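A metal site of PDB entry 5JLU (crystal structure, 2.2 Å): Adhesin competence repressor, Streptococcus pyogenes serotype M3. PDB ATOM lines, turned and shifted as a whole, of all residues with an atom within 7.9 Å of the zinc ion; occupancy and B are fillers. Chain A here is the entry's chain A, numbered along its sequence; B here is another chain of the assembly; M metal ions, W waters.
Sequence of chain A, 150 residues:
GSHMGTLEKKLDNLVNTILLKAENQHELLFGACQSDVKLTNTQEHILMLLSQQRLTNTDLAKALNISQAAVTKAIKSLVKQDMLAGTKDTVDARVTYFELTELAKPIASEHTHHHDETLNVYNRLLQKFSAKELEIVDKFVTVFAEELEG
The backbone carbonyl oxygen (O) of His 115 sits at hydrogen-bond distance from the side-chain hydroxyl (OG1) of Thr 118, at 2.7 Å. The side-chain carboxylate (OD1) of Asp 12 of chain B sits at hydrogen-bond distance from a ring nitrogen (ND1) of His 115 (2.8 Å).
Within 4 Å of the zinc ion: His 45, His 111 and His 115. The nearest printed residue that does not touch the zinc ion is Asn 16 of chain B (4.2 Å).
The zinc ion is bound by water W3, 2.0 Å away. NE2 of His 115 binds the zinc ion. The zinc ion is bound by NE2 of His 45, 2.1 Å away. NE2 of His 111 is bound to the zinc ion (2.1 Å). Water W1 binds the zinc ion, at 2.2 Å. Water W2 is bound to the zinc ion. The zinc ion has six donor atoms within binding distance.
Water W2 bridges OE1 of Glu 44 (2.5 Å) and OD1 of Asn 41 (2.6 Å).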
ATOM      1  N   THR A  40      24.383  -4.578 -29.881  1.00  0.00           N
ATOM      2  CA  THR A  40      23.290  -5.553 -29.865  1.00  0.00           C
ATOM      3  C   THR A  40      23.434  -6.486 -28.684  1.00  0.00           C
ATOM      4  O   THR A  40      24.483  -6.591 -28.108  1.00  0.00           O
ATOM      5  CB  THR A  40      23.335  -6.428 -31.112  1.00  0.00           C
ATOM      6  OG1 THR A  40      24.598  -7.159 -31.125  1.00  0.00           O
ATOM      7  CG2 THR A  40      23.217  -5.507 -32.343  1.00  0.00           C
ATOM      8  N   ASN A  41      22.381  -7.205 -28.375  1.00  0.00           N
ATOM      9  CA  ASN A  41      22.433  -8.153 -27.274  1.00  0.00           C
ATOM     10  C   ASN A  41      23.476  -9.239 -27.548  1.00  0.00           C
ATOM     11  O   ASN A  41      24.174  -9.667 -26.624  1.00  0.00           O
ATOM     12  CB  ASN A  41      21.071  -8.790 -27.039  1.00  0.00           C
ATOM     13  CG  ASN A  41      20.062  -7.770 -26.527  1.00  0.00           C
ATOM     14  OD1 ASN A  41      20.041  -7.431 -25.332  1.00  0.00           O
ATOM     15  ND2 ASN A  41      19.252  -7.240 -27.423  1.00  0.00           N
ATOM     16  N   THR A  42      23.626  -9.579 -28.801  1.00  0.00           N
ATOM     17  CA  THR A  42      24.556 -10.606 -29.183  1.00  0.00           C
ATOM     18  C   THR A  42      25.919 -10.126 -28.813  1.00  0.00           C
ATOM     19  O   THR A  42      26.689 -10.843 -28.239  1.00  0.00           O
ATOM     20  CB  THR A  42      24.508 -10.847 -30.698  1.00  0.00           C
ATOM     21  OG1 THR A  42      23.228 -11.316 -31.046  1.00  0.00           O
ATOM     22  CG2 THR A  42      25.518 -11.849 -31.146  1.00  0.00           C
ATOM     23  N   GLU A  44      26.688  -7.741 -26.657  1.00  0.00           N
ATOM     24  CA  GLU A  44      26.904  -7.627 -25.203  1.00  0.00           C
ATOM     25  C   GLU A  44      27.159  -8.995 -24.553  1.00  0.00           C
ATOM     26  O   GLU A  44      27.888  -9.066 -23.555  1.00  0.00           O
ATOM     27  CB  GLU A  44      25.682  -7.041 -24.475  1.00  0.00           C
ATOM     28  CG  GLU A  44      25.446  -5.581 -24.721  1.00  0.00           C
ATOM     29  CD  GLU A  44      24.070  -5.073 -24.203  1.00  0.00           C
ATOM     30  OE1 GLU A  44      23.031  -5.770 -24.279  1.00  0.00           O
ATOM     31  OE2 GLU A  44      24.023  -3.989 -23.656  1.00  0.00           O
ATOM     32  N   HIS A  45      26.542 -10.064 -25.082  1.00  0.00           N
ATOM     33  CA  HIS A  45      26.713 -11.373 -24.522  1.00  0.00           C
ATOM     34  C   HIS A  45      28.022 -12.029 -24.957  1.00  0.00           C
ATOM     35  O   HIS A  45      28.580 -12.802 -24.193  1.00  0.00           O
ATOM     36  CB  HIS A  45      25.478 -12.261 -24.706  1.00  0.00           C
ATOM     37  CG  HIS A  45      24.457 -11.850 -23.736  1.00  0.00           C
ATOM     38  ND1 HIS A  45      24.345 -12.444 -22.508  1.00  0.00           N
ATOM     39  CD2 HIS A  45      23.688 -10.739 -23.698  1.00  0.00           C
ATOM     40  CE1 HIS A  45      23.500 -11.765 -21.771  1.00  0.00           C
ATOM     41  NE2 HIS A  45      23.078 -10.732 -22.476  1.00  0.00           N
ATOM     42  N   MET A  48      30.152 -10.316 -22.471  1.00  0.00           N
ATOM     43  CA  MET A  48      29.989 -11.048 -21.172  1.00  0.00           C
ATOM     44  C   MET A  48      30.835 -12.350 -21.106  1.00  0.00           C
ATOM     45  O   MET A  48      31.545 -12.629 -20.122  1.00  0.00           O
ATOM     46  CB  MET A  48      28.509 -11.329 -20.888  1.00  0.00           C
ATOM     47  CG  MET A  48      28.207 -12.143 -19.646  1.00  0.00           C
ATOM     48  SD  MET A  48      26.437 -12.250 -19.293  1.00  0.00           S
ATOM     49  CE  MET A  48      26.195 -10.702 -18.514  1.00  0.00           C
ATOM     50  N   HIS A 111      26.900  -4.214 -18.102  1.00  0.00           N
ATOM     51  CA  HIS A 111      25.921  -5.140 -18.623  1.00  0.00           C
ATOM     52  C   HIS A 111      25.841  -6.359 -17.690  1.00  0.00           C
ATOM     53  O   HIS A 111      24.761  -6.807 -17.379  1.00  0.00           O
ATOM     54  CB  HIS A 111      26.298  -5.543 -20.043  1.00  0.00           C
ATOM     55  CG  HIS A 111      25.465  -6.628 -20.581  1.00  0.00           C
ATOM     56  ND1 HIS A 111      25.918  -7.926 -20.727  1.00  0.00           N
ATOM     57  CD2 HIS A 111      24.161  -6.627 -20.956  1.00  0.00           C
ATOM     58  CE1 HIS A 111      24.943  -8.655 -21.223  1.00  0.00           C
ATOM     59  NE2 HIS A 111      23.859  -7.887 -21.351  1.00  0.00           N
ATOM     60  N   THR A 112      26.973  -6.815 -17.171  1.00  0.00           N
ATOM     61  CA  THR A 112      26.984  -7.938 -16.247  1.00  0.00           C
ATOM     62  C   THR A 112      26.272  -7.608 -14.942  1.00  0.00           C
ATOM     63  O   THR A 112      25.667  -8.478 -14.331  1.00  0.00           O
ATOM     64  CB  THR A 112      28.410  -8.380 -15.972  1.00  0.00           C
ATOM     65  OG1 THR A 112      28.926  -8.994 -17.130  1.00  0.00           O
ATOM     66  CG2 THR A 112      28.520  -9.388 -14.826  1.00  0.00           C
ATOM     67  N   HIS A 114      23.783  -5.298 -14.555  1.00  0.00           N
ATOM     68  CA  HIS A 114      22.333  -5.327 -14.869  1.00  0.00           C
ATOM     69  C   HIS A 114      21.725  -6.752 -14.936  1.00  0.00           C
ATOM     70  O   HIS A 114      20.570  -6.937 -14.552  1.00  0.00           O
ATOM     71  CB  HIS A 114      22.009  -4.555 -16.161  1.00  0.00           C
ATOM     72  CG  HIS A 114      22.124  -3.051 -16.027  1.00  0.00           C
ATOM     73  ND1 HIS A 114      21.623  -2.179 -16.976  1.00  0.00           N
ATOM     74  CD2 HIS A 114      22.652  -2.281 -15.044  1.00  0.00           C
ATOM     75  CE1 HIS A 114      21.844  -0.933 -16.574  1.00  0.00           C
ATOM     76  NE2 HIS A 114      22.469  -0.969 -15.408  1.00  0.00           N
ATOM     77  N   HIS A 115      22.471  -7.736 -15.447  1.00  0.00           N
ATOM     78  CA  HIS A 115      22.073  -9.152 -15.381  1.00  0.00           C
ATOM     79  C   HIS A 115      21.974  -9.650 -13.908  1.00  0.00           C
ATOM     80  O   HIS A 115      21.021 -10.376 -13.592  1.00  0.00           O
ATOM     81  CB  HIS A 115      22.911 -10.078 -16.287  1.00  0.00           C
ATOM     82  CG  HIS A 115      22.420 -10.041 -17.698  1.00  0.00           C
ATOM     83  ND1 HIS A 115      21.334 -10.791 -18.122  1.00  0.00           N
ATOM     84  CD2 HIS A 115      22.767  -9.256 -18.747  1.00  0.00           C
ATOM     85  CE1 HIS A 115      21.029 -10.459 -19.358  1.00  0.00           C
ATOM     86  NE2 HIS A 115      21.919  -9.577 -19.781  1.00  0.00           N
ATOM     87  N   THR A 118      18.879  -8.322 -12.404  1.00  0.00           N
ATOM     88  CA  THR A 118      17.647  -8.953 -12.884  1.00  0.00           C
ATOM     89  C   THR A 118      17.477 -10.361 -12.234  1.00  0.00           C
ATOM     90  O   THR A 118      16.371 -10.823 -12.113  1.00  0.00           O
ATOM     91  CB  THR A 118      17.567  -9.106 -14.421  1.00  0.00           C
ATOM     92  OG1 THR A 118      18.614  -9.981 -14.836  1.00  0.00           O
ATOM     93  CG2 THR A 118      17.749  -7.776 -15.155  1.00  0.00           C
ATOM     94  N   ASP B  12      16.978 -16.227 -16.809  1.00  0.00           N
ATOM     95  CA  ASP B  12      17.909 -15.280 -17.385  1.00  0.00           C
ATOM     96  C   ASP B  12      18.266 -15.789 -18.782  1.00  0.00           C
ATOM     97  O   ASP B  12      18.168 -15.016 -19.757  1.00  0.00           O
ATOM     98  CB  ASP B  12      19.148 -15.182 -16.512  1.00  0.00           C
ATOM     99  CG  ASP B  12      20.139 -14.100 -16.963  1.00  0.00           C
ATOM    100  OD1 ASP B  12      19.733 -12.949 -17.207  1.00  0.00           O
ATOM    101  OD2 ASP B  12      21.347 -14.385 -17.040  1.00  0.00           O
ATOM    102  N   VAL B  15      15.297 -15.443 -21.258  1.00  0.00           N
ATOM    103  CA  VAL B  15      15.246 -14.119 -21.810  1.00  0.00           C
ATOM    104  C   VAL B  15      16.336 -13.868 -22.917  1.00  0.00           C
ATOM    105  O   VAL B  15      16.085 -13.210 -23.971  1.00  0.00           O
ATOM    106  CB  VAL B  15      15.266 -13.115 -20.656  1.00  0.00           C
ATOM    107  CG1 VAL B  15      15.372 -11.664 -21.115  1.00  0.00           C
ATOM    108  CG2 VAL B  15      14.018 -13.268 -19.818  1.00  0.00           C
ATOM    109  N   ASN B  16      17.545 -14.400 -22.684  1.00  0.00           N
ATOM    110  CA  ASN B  16      18.660 -14.181 -23.591  1.00  0.00           C
ATOM    111  C   ASN B  16      18.437 -14.876 -24.883  1.00  0.00           C
ATOM    112  O   ASN B  16      18.788 -14.284 -25.937  1.00  0.00           O
ATOM    113  CB  ASN B  16      20.046 -14.622 -22.993  1.00  0.00           C
ATOM    114  CG  ASN B  16      20.494 -13.711 -21.852  1.00  0.00           C
ATOM    115  OD1 ASN B  16      19.992 -12.563 -21.692  1.00  0.00           O
ATOM    116  ND2 ASN B  16      21.383 -14.192 -21.042  1.00  0.00           N
ATOM    117  N   LEU B  19      16.050 -12.895 -26.878  1.00  0.00           N
ATOM    118  CA  LEU B  19      16.715 -11.741 -27.483  1.00  0.00           C
ATOM    119  C   LEU B  19      17.662 -12.193 -28.636  1.00  0.00           C
ATOM    120  O   LEU B  19      17.610 -11.621 -29.764  1.00  0.00           O
ATOM    121  CB  LEU B  19      17.410 -10.891 -26.424  1.00  0.00           C
ATOM    122  CG  LEU B  19      16.507 -10.238 -25.337  1.00  0.00           C
ATOM    123  CD1 LEU B  19      17.287  -9.473 -24.285  1.00  0.00           C
ATOM    124  CD2 LEU B  19      15.529  -9.285 -26.003  1.00  0.00           C
ATOM    125  N   LEU B  20      18.457 -13.238 -28.408  1.00  0.00           N
ATOM    126  CA  LEU B  20      19.427 -13.677 -29.408  1.00  0.00           C
ATOM    127  C   LEU B  20      18.837 -14.253 -30.685  1.00  0.00           C
ATOM    128  O   LEU B  20      19.425 -14.114 -31.794  1.00  0.00           O
ATOM    129  CB  LEU B  20      20.394 -14.698 -28.854  1.00  0.00           C
ATOM    130  CG  LEU B  20      21.213 -14.174 -27.674  1.00  0.00           C
ATOM    131  CD1 LEU B  20      21.962 -15.370 -27.080  1.00  0.00           C
ATOM    132  CD2 LEU B  20      22.125 -13.049 -28.034  1.00  0.00           C
HETATM  133 ZN    ZN M   1      22.094  -8.984 -21.792  1.00  0.00          ZN
HETATM  134  O   HOH W   1      20.217  -9.923 -22.329  1.00  0.00           O
HETATM  135  O   HOH W   2      22.054  -8.024 -23.776  1.00  0.00           O
HETATM  136  O   HOH W   3      20.949  -7.423 -21.177  1.00  0.00           O
